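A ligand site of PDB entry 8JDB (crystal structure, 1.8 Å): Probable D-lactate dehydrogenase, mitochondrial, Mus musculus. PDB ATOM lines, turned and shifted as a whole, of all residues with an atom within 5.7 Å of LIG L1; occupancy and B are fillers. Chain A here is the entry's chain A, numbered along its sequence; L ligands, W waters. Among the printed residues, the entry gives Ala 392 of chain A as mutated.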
ATOM      1  N   GLU A  45       6.478  13.701  -1.443  1.00  0.00           N
ATOM      2  CA  GLU A  45       5.401  13.608  -2.414  1.00  0.00           C
ATOM      3  C   GLU A  45       4.340  14.688  -2.253  1.00  0.00           C
ATOM      4  O   GLU A  45       3.412  14.748  -3.070  1.00  0.00           O
ATOM      5  CB  GLU A  45       4.777  12.206  -2.347  1.00  0.00           C
ATOM      6  CG  GLU A  45       5.692  11.151  -2.957  1.00  0.00           C
ATOM      7  CD  GLU A  45       5.964  11.400  -4.441  1.00  0.00           C
ATOM      8  OE1 GLU A  45       5.024  11.275  -5.255  1.00  0.00           O
ATOM      9  OE2 GLU A  45       7.102  11.761  -4.807  1.00  0.00           O
ATOM     10  N   SER A  46       4.483  15.564  -1.258  1.00  0.00           N
ATOM     11  CA  SER A  46       3.569  16.663  -0.982  1.00  0.00           C
ATOM     12  C   SER A  46       3.832  17.862  -1.891  1.00  0.00           C
ATOM     13  O   SER A  46       4.869  17.953  -2.553  1.00  0.00           O
ATOM     14  CB  SER A  46       3.702  17.122   0.464  1.00  0.00           C
ATOM     15  OG  SER A  46       4.846  17.942   0.629  1.00  0.00           O
ATOM     16  N   THR A  86       8.557   9.592   0.598  1.00  0.00           N
ATOM     17  CA  THR A  86       7.139   9.491   0.262  1.00  0.00           C
ATOM     18  C   THR A  86       6.243  10.228   1.258  1.00  0.00           C
ATOM     19  O   THR A  86       5.013  10.086   1.194  1.00  0.00           O
ATOM     20  CB  THR A  86       6.690   8.014   0.157  1.00  0.00           C
ATOM     21  OG1 THR A  86       6.665   7.376   1.446  1.00  0.00           O
ATOM     22  CG2 THR A  86       7.613   7.223  -0.768  1.00  0.00           C
ATOM     23  N   GLY A  87       6.819  11.010   2.158  1.00  0.00           N
ATOM     24  CA  GLY A  87       6.038  11.676   3.189  1.00  0.00           C
ATOM     25  C   GLY A  87       5.128  12.754   2.634  1.00  0.00           C
ATOM     26  O   GLY A  87       5.181  13.137   1.466  1.00  0.00           O
ATOM     27  N   VAL A  88       4.291  13.274   3.535  1.00  0.00           N
ATOM     28  CA  VAL A  88       3.131  14.076   3.188  1.00  0.00           C
ATOM     29  C   VAL A  88       3.263  15.547   3.615  1.00  0.00           C
ATOM     30  O   VAL A  88       2.508  16.396   3.093  1.00  0.00           O
ATOM     31  CB  VAL A  88       1.857  13.458   3.812  1.00  0.00           C
ATOM     32  CG1 VAL A  88       0.577  14.173   3.389  1.00  0.00           C
ATOM     33  CG2 VAL A  88       1.792  12.001   3.475  1.00  0.00           C
ATOM     34  N   GLY A 146       0.113   3.252   1.299  1.00  0.00           N
ATOM     35  CA  GLY A 146       0.000   2.987  -0.123  1.00  0.00           C
ATOM     36  C   GLY A 146       1.329   2.940  -0.848  1.00  0.00           C
ATOM     37  O   GLY A 146       1.483   2.183  -1.811  1.00  0.00           O
ATOM     38  N   GLU A 264     -12.264   0.469   3.916  1.00  0.00           N
ATOM     39  CA  GLU A 264     -11.758   1.684   3.290  1.00  0.00           C
ATOM     40  C   GLU A 264     -12.862   2.391   2.535  1.00  0.00           C
ATOM     41  O   GLU A 264     -13.639   1.757   1.818  1.00  0.00           O
ATOM     42  CB  GLU A 264     -10.617   1.346   2.328  1.00  0.00           C
ATOM     43  CG  GLU A 264      -9.383   0.849   3.076  1.00  0.00           C
ATOM     44  CD  GLU A 264      -8.693   1.972   3.824  1.00  0.00           C
ATOM     45  OE1 GLU A 264      -8.602   3.081   3.272  1.00  0.00           O
ATOM     46  OE2 GLU A 264      -8.245   1.725   4.969  1.00  0.00           O
ATOM     47  N   ARG A 334      -6.458   0.819  -4.506  1.00  0.00           N
ATOM     48  CA  ARG A 334      -6.628   1.625  -3.306  1.00  0.00           C
ATOM     49  C   ARG A 334      -5.307   2.246  -2.897  1.00  0.00           C
ATOM     50  O   ARG A 334      -5.242   3.436  -2.582  1.00  0.00           O
ATOM     51  CB  ARG A 334      -7.208   0.769  -2.181  1.00  0.00           C
ATOM     52  CG  ARG A 334      -7.116   1.410  -0.789  1.00  0.00           C
ATOM     53  CD  ARG A 334      -7.879   2.740  -0.708  1.00  0.00           C
ATOM     54  NE  ARG A 334      -7.651   3.389   0.587  1.00  0.00           N
ATOM     55  CZ  ARG A 334      -6.734   4.332   0.785  1.00  0.00           C
ATOM     56  NH1 ARG A 334      -5.973   4.748  -0.219  1.00  0.00           N
ATOM     57  NH2 ARG A 334      -6.584   4.859   2.001  1.00  0.00           N
ATOM     58  N   HIS A 335      -4.240   1.448  -2.892  1.00  0.00           N
ATOM     59  CA  HIS A 335      -2.941   1.990  -2.478  1.00  0.00           C
ATOM     60  C   HIS A 335      -2.480   3.116  -3.388  1.00  0.00           C
ATOM     61  O   HIS A 335      -1.763   4.021  -2.926  1.00  0.00           O
ATOM     62  CB  HIS A 335      -1.903   0.867  -2.428  1.00  0.00           C
ATOM     63  CG  HIS A 335      -2.031   0.004  -1.215  1.00  0.00           C
ATOM     64  ND1 HIS A 335      -1.665  -1.328  -1.213  1.00  0.00           N
ATOM     65  CD2 HIS A 335      -2.455   0.284   0.043  1.00  0.00           C
ATOM     66  CE1 HIS A 335      -1.868  -1.833  -0.009  1.00  0.00           C
ATOM     67  NE2 HIS A 335      -2.341  -0.867   0.772  1.00  0.00           N
ATOM     68  N   ALA A 337      -4.468   5.353  -4.809  1.00  0.00           N
ATOM     69  CA  ALA A 337      -5.517   6.357  -4.911  1.00  0.00           C
ATOM     70  C   ALA A 337      -4.948   7.761  -5.038  1.00  0.00           C
ATOM     71  O   ALA A 337      -5.463   8.592  -5.802  1.00  0.00           O
ATOM     72  CB  ALA A 337      -6.444   6.273  -3.708  1.00  0.00           C
ATOM     73  N   TRP A 338      -3.883   8.059  -4.296  1.00  0.00           N
ATOM     74  CA  TRP A 338      -3.253   9.371  -4.391  1.00  0.00           C
ATOM     75  C   TRP A 338      -2.869   9.697  -5.827  1.00  0.00           C
ATOM     76  O   TRP A 338      -3.181  10.776  -6.346  1.00  0.00           O
ATOM     77  CB  TRP A 338      -2.024   9.431  -3.484  1.00  0.00           C
ATOM     78  CG  TRP A 338      -1.174  10.651  -3.640  1.00  0.00           C
ATOM     79  CD1 TRP A 338       0.041  10.724  -4.258  1.00  0.00           C
ATOM     80  CD2 TRP A 338      -1.440  11.963  -3.114  1.00  0.00           C
ATOM     81  NE1 TRP A 338       0.535  12.007  -4.176  1.00  0.00           N
ATOM     82  CE2 TRP A 338      -0.343  12.788  -3.481  1.00  0.00           C
ATOM     83  CE3 TRP A 338      -2.490  12.530  -2.385  1.00  0.00           C
ATOM     84  CZ2 TRP A 338      -0.283  14.138  -3.145  1.00  0.00           C
ATOM     85  CZ3 TRP A 338      -2.421  13.876  -2.053  1.00  0.00           C
ATOM     86  CH2 TRP A 338      -1.326  14.664  -2.429  1.00  0.00           C
ATOM     87  N   SER A 352      -2.993  17.017   1.104  1.00  0.00           N
ATOM     88  CA  SER A 352      -3.836  16.015   1.739  1.00  0.00           C
ATOM     89  C   SER A 352      -4.069  16.382   3.189  1.00  0.00           C
ATOM     90  O   SER A 352      -3.116  16.700   3.912  1.00  0.00           O
ATOM     91  CB  SER A 352      -3.226  14.614   1.675  1.00  0.00           C
ATOM     92  OG  SER A 352      -4.120  13.638   2.251  1.00  0.00           O
ATOM     93  N   ASP A 354      -5.895  14.798   6.892  1.00  0.00           N
ATOM     94  CA  ASP A 354      -5.672  13.532   7.575  1.00  0.00           C
ATOM     95  C   ASP A 354      -6.350  13.484   8.944  1.00  0.00           C
ATOM     96  O   ASP A 354      -5.846  12.812   9.844  1.00  0.00           O
ATOM     97  CB  ASP A 354      -4.161  13.280   7.747  1.00  0.00           C
ATOM     98  CG  ASP A 354      -3.818  11.884   8.270  1.00  0.00           C
ATOM     99  OD1 ASP A 354      -4.533  10.895   7.968  1.00  0.00           O
ATOM    100  OD2 ASP A 354      -2.813  11.765   9.008  1.00  0.00           O
ATOM    101  N   VAL A 383     -10.759   9.817   0.428  1.00  0.00           N
ATOM    102  CA  VAL A 383     -10.457   8.414   0.596  1.00  0.00           C
ATOM    103  C   VAL A 383     -10.072   8.224   2.058  1.00  0.00           C
ATOM    104  O   VAL A 383      -9.576   9.143   2.701  1.00  0.00           O
ATOM    105  CB  VAL A 383      -9.334   7.967  -0.366  1.00  0.00           C
ATOM    106  CG1 VAL A 383      -7.983   8.591   0.074  1.00  0.00           C
ATOM    107  CG2 VAL A 383      -9.243   6.452  -0.424  1.00  0.00           C
ATOM    108  N   GLY A 384     -10.314   7.035   2.613  1.00  0.00           N
ATOM    109  CA  GLY A 384      -9.936   6.990   4.007  1.00  0.00           C
ATOM    110  C   GLY A 384     -10.005   5.707   4.794  1.00  0.00           C
ATOM    111  O   GLY A 384     -10.822   4.828   4.534  1.00  0.00           O
ATOM    112  N   HIS A 385      -9.113   5.629   5.791  1.00  0.00           N
ATOM    113  CA  HIS A 385      -9.123   4.534   6.765  1.00  0.00           C
ATOM    114  C   HIS A 385     -10.232   4.790   7.792  1.00  0.00           C
ATOM    115  O   HIS A 385      -9.989   5.047   8.971  1.00  0.00           O
ATOM    116  CB  HIS A 385      -7.778   4.429   7.471  1.00  0.00           C
ATOM    117  CG  HIS A 385      -6.591   4.474   6.553  1.00  0.00           C
ATOM    118  ND1 HIS A 385      -6.389   3.545   5.546  1.00  0.00           N
ATOM    119  CD2 HIS A 385      -5.506   5.283   6.537  1.00  0.00           C
ATOM    120  CE1 HIS A 385      -5.241   3.807   4.939  1.00  0.00           C
ATOM    121  NE2 HIS A 385      -4.684   4.854   5.516  1.00  0.00           N
ATOM    122  N   ALA A 392      -8.732  11.086   4.457  1.00  0.00           N
ATOM    123  CA  ALA A 392      -7.943  12.083   3.748  1.00  0.00           C
ATOM    124  C   ALA A 392      -8.809  12.822   2.733  1.00  0.00           C
ATOM    125  O   ALA A 392      -9.609  12.198   2.036  1.00  0.00           O
ATOM    126  CB  ALA A 392      -6.760  11.444   3.017  1.00  0.00           C
ATOM    127  N   ILE A 394      -8.100  14.926  -0.546  1.00  0.00           N
ATOM    128  CA  ILE A 394      -7.039  15.184  -1.522  1.00  0.00           C
ATOM    129  C   ILE A 394      -7.450  16.412  -2.324  1.00  0.00           C
ATOM    130  O   ILE A 394      -8.462  16.374  -3.033  1.00  0.00           O
ATOM    131  CB  ILE A 394      -6.802  13.960  -2.423  1.00  0.00           C
ATOM    132  CG1 ILE A 394      -6.310  12.780  -1.572  1.00  0.00           C
ATOM    133  CG2 ILE A 394      -5.828  14.301  -3.547  1.00  0.00           C
ATOM    134  CD1 ILE A 394      -6.354  11.447  -2.305  1.00  0.00           C
ATOM    135  N   GLU A 429      -2.272   9.800  10.892  1.00  0.00           N
ATOM    136  CA  GLU A 429      -1.123   8.980  10.527  1.00  0.00           C
ATOM    137  C   GLU A 429      -0.013   9.722   9.778  1.00  0.00           C
ATOM    138  O   GLU A 429       1.152   9.314   9.870  1.00  0.00           O
ATOM    139  CB  GLU A 429      -1.586   7.784   9.658  1.00  0.00           C
ATOM    140  CG  GLU A 429      -2.303   8.223   8.372  1.00  0.00           C
ATOM    141  CD  GLU A 429      -2.755   7.074   7.469  1.00  0.00           C
ATOM    142  OE1 GLU A 429      -2.535   5.871   7.783  1.00  0.00           O
ATOM    143  OE2 GLU A 429      -3.270   7.401   6.368  1.00  0.00           O
ATOM    144  N   HIS A 430      -0.343  10.772   9.003  1.00  0.00           N
ATOM    145  CA  HIS A 430       0.674  11.381   8.136  1.00  0.00           C
ATOM    146  C   HIS A 430       1.712  12.162   8.930  1.00  0.00           C
ATOM    147  O   HIS A 430       2.873  12.246   8.523  1.00  0.00           O
ATOM    148  CB  HIS A 430       0.039  12.333   7.134  1.00  0.00           C
ATOM    149  CG  HIS A 430      -0.811  11.639   6.117  1.00  0.00           C
ATOM    150  ND1 HIS A 430      -1.764  12.309   5.377  1.00  0.00           N
ATOM    151  CD2 HIS A 430      -0.851  10.357   5.712  1.00  0.00           C
ATOM    152  CE1 HIS A 430      -2.359  11.449   4.564  1.00  0.00           C
ATOM    153  NE2 HIS A 430      -1.826  10.258   4.744  1.00  0.00           N
HETATM  154  C1  LIG L   1      -3.874   7.057   1.573  1.00  0.00           C
HETATM  155  C2  LIG L   1      -3.007   8.297   1.759  1.00  0.00           C
HETATM  156  C3  LIG L   1      -3.540   9.413   0.880  1.00  0.00           C
HETATM  157  C4  LIG L   1      -2.650  10.654   0.982  1.00  0.00           C
HETATM  158  C5  LIG L   1      -1.283  10.449   0.326  1.00  0.00           C
HETATM  159  C6  LIG L   1      -0.483  11.740   0.493  1.00  0.00           C
HETATM  160  C7  LIG L   1       0.889  11.622  -0.186  1.00  0.00           C
HETATM  161  C8  LIG L   1       1.523  13.017  -0.224  1.00  0.00           C
HETATM  162  O1  LIG L   1      -3.093   8.616   3.126  1.00  0.00           O
HETATM  163  O2  LIG L   1      -3.786   6.369   0.520  1.00  0.00           O
HETATM  164  O3  LIG L   1      -4.669   6.733   2.495  1.00  0.00           O
HETATM  165  P1  LG2 L   2      10.309  10.445   4.173  1.00  0.00           P
HETATM  166  O1  LG2 L   2       9.509  11.374   3.357  1.00  0.00           O
HETATM  167  O2  LG2 L   2      11.692  10.037   3.701  1.00  0.00           O
HETATM  168  O3  LG2 L   2      10.444  11.063   5.627  1.00  0.00           O
HETATM  169  C1  LG2 L   2       9.270  11.367   6.413  1.00  0.00           C
HETATM  170  C2  LG2 L   2       9.678  12.012   7.712  1.00  0.00           C
HETATM  171  O4  LG2 L   2      10.322  11.047   8.567  1.00  0.00           O
HETATM  172  C3  LG2 L   2      10.669  13.171   7.581  1.00  0.00           C
HETATM  173  O5  LG2 L   2      10.419  14.166   8.564  1.00  0.00           O
HETATM  174  C4  LG2 L   2      12.030  12.481   7.752  1.00  0.00           C
HETATM  175  O6  LG2 L   2      13.027  13.331   8.302  1.00  0.00           O
HETATM  176  C5  LG2 L   2      11.684  11.391   8.769  1.00  0.00           C
HETATM  177  N1  LG2 L   2      12.458  10.152   8.644  1.00  0.00           N
HETATM  178  C6  LG2 L   2      12.491   9.273   7.597  1.00  0.00           C
HETATM  179  N2  LG2 L   2      13.233   8.221   7.812  1.00  0.00           N
HETATM  180  C7  LG2 L   2      13.686   8.386   9.115  1.00  0.00           C
HETATM  181  C8  LG2 L   2      14.532   7.611   9.929  1.00  0.00           C
HETATM  182  N3  LG2 L   2      15.065   6.438   9.578  1.00  0.00           N
HETATM  183  N4  LG2 L   2      14.804   8.096  11.161  1.00  0.00           N
HETATM  184  C9  LG2 L   2      14.267   9.259  11.542  1.00  0.00           C
HETATM  185  N5  LG2 L   2      13.466  10.066  10.854  1.00  0.00           N
HETATM  186  C10 LG2 L   2      13.223   9.580   9.629  1.00  0.00           C
HETATM  187  N6  LG2 L   2       1.167   7.257   5.241  1.00  0.00           N
HETATM  188  C11 LG2 L   2       0.388   6.618   6.159  1.00  0.00           C
HETATM  189  O7  LG2 L   2       0.623   6.725   7.383  1.00  0.00           O
HETATM  190  N7  LG2 L   2      -0.661   5.825   5.741  1.00  0.00           N
HETATM  191  C12 LG2 L   2      -1.030   5.584   4.418  1.00  0.00           C
HETATM  192  O8  LG2 L   2      -2.002   4.869   4.181  1.00  0.00           O
HETATM  193  C13 LG2 L   2      -0.189   6.264   3.443  1.00  0.00           C
HETATM  194  N8  LG2 L   2      -0.454   6.091   2.142  1.00  0.00           N
HETATM  195  C14 LG2 L   2       0.350   6.752   1.220  1.00  0.00           C
HETATM  196  C15 LG2 L   2       0.096   6.581  -0.140  1.00  0.00           C
HETATM  197  C16 LG2 L   2       0.880   7.217  -1.094  1.00  0.00           C
HETATM  198  C17 LG2 L   2       0.573   7.027  -2.561  1.00  0.00           C
HETATM  199  C18 LG2 L   2       1.953   8.037  -0.688  1.00  0.00           C
HETATM  200  C19 LG2 L   2       2.822   8.748  -1.695  1.00  0.00           C
HETATM  201  C20 LG2 L   2       2.215   8.203   0.668  1.00  0.00           C
HETATM  202  C21 LG2 L   2       1.422   7.571   1.627  1.00  0.00           C
HETATM  203  N9  LG2 L   2       1.694   7.689   3.012  1.00  0.00           N
HETATM  204  C22 LG2 L   2       0.881   7.087   3.944  1.00  0.00           C
HETATM  205  C23 LG2 L   2       2.746   8.618   3.494  1.00  0.00           C
HETATM  206  C24 LG2 L   2       4.139   8.010   3.602  1.00  0.00           C
HETATM  207  O9  LG2 L   2       4.266   6.893   2.732  1.00  0.00           O
HETATM  208  C25 LG2 L   2       4.412   7.629   5.056  1.00  0.00           C
HETATM  209  O10 LG2 L   2       4.352   8.798   5.864  1.00  0.00           O
HETATM  210  C26 LG2 L   2       5.777   6.958   5.237  1.00  0.00           C
HETATM  211  O11 LG2 L   2       5.881   6.526   6.597  1.00  0.00           O
HETATM  212  C27 LG2 L   2       6.915   7.892   4.890  1.00  0.00           C
HETATM  213  O12 LG2 L   2       8.152   7.146   4.887  1.00  0.00           O
HETATM  214  P2  LG2 L   2       9.375   7.651   4.046  1.00  0.00           P
HETATM  215  O13 LG2 L   2      10.632   6.891   4.459  1.00  0.00           O
HETATM  216  O14 LG2 L   2       9.045   7.592   2.575  1.00  0.00           O
HETATM  217  O15 LG2 L   2       9.446   9.165   4.529  1.00  0.00           O
HETATM  218  O   HOH W   1      -3.038   3.503   0.707  1.00  0.00           O
HETATM  219  O   HOH W   2      -3.063   6.472  -2.106  1.00  0.00           O
HETATM  220  O   HOH W   3      -4.873   9.320   5.704  1.00  0.00           O
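Residues that only touch LIG L1: Glu 45 (3.8 Å), Val 88 (3.8 Å), Trp 338 (3.6 Å), Ser 352 (3.6 Å) and His 385 (3.6 Å). Eight residues have an atom within 4 Å of LIG L1: Glu 45, Val 88, Arg 334, Trp 338, Ser 352, His 385, Glu 429 and His 430.
Water W2 lies within hydrogen-bond range of an oxygen (O2) of LIG L1 (2.7 Å), the backbone NH of Trp 338 (2.8 Å), the backbone carbonyl oxygen of His 335 (2.9 Å) and the backbone NH of Ala 337 (3.2 Å). Water W1 lies within hydrogen-bond range of an oxygen (O2) of LIG L1 (3.0 Å), the backbone NH of Gly 146 (3.2 Å) and the guanidinium group of Arg 334 (3.3 Å). Water W3 lies within hydrogen-bond range of the side-chain carboxylate (OE2) of Glu 429 (2.6 Å), the side-chain carboxylate (OD1) of Asp 354 (2.8 Å), an oxygen (O1) of LIG L1 (3.2 Å) and a ring nitrogen (NE2) of His 430 (3.3 Å).
A ring nitrogen (NE2) of His 430 lies within hydrogen-bond range of an oxygen (O1) of LIG L1, at 2.6 Å. O3 of LIG L1 lies within salt-bridge range of NH2 of Arg 334 (2.7 Å). An oxygen (O1) of LIG L1 lies within hydrogen-bond range of the side-chain carboxylate (OE2) of Glu 429 (3.5 Å). N7 of LG2 L2 is in hydrogen-bond range of OE1 of Glu 429 (2.8 Å). A ring nitrogen (NE2) of His 385 sits at hydrogen-bond distance from an oxygen (O8) of LG2 L2, 3.0 Å away. O1 of LG2 L2 sits at hydrogen-bond distance from N of Gly 87. N of Thr 86 sits at hydrogen-bond distance from O14 of LG2 L2 (2.9 Å). The side-chain hydroxyl (OG1) of Thr 86 lies within hydrogen-bond range of an oxygen (O14) of LG2 L2, at 2.6 Å. The backbone NH of Gly 146 sits at hydrogen-bond distance from a nitrogen (N8) of LG2 L2, at 3.0 Å.
N of His 430 sits at hydrogen-bond distance from OD2 of Asp 354 (2.7 Å). The guanidinium group (NE) of Arg 334 lies within salt-bridge range of the side-chain carboxylate (OE1) of Glu 264 (2.9 Å). OE2 of Glu 429 sits at hydrogen-bond distance from NE2 of His 385 (3.0 Å). The backbone NH of Glu 429 sits at hydrogen-bond distance from the side-chain carboxylate of Asp 354 (2.8 Å). The side-chain carboxylate (OE2) of Glu 264 sits at hydrogen-bond distance from a ring nitrogen (ND1) of His 385. O of Gly 87 lies within hydrogen-bond range of N of Glu 45.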
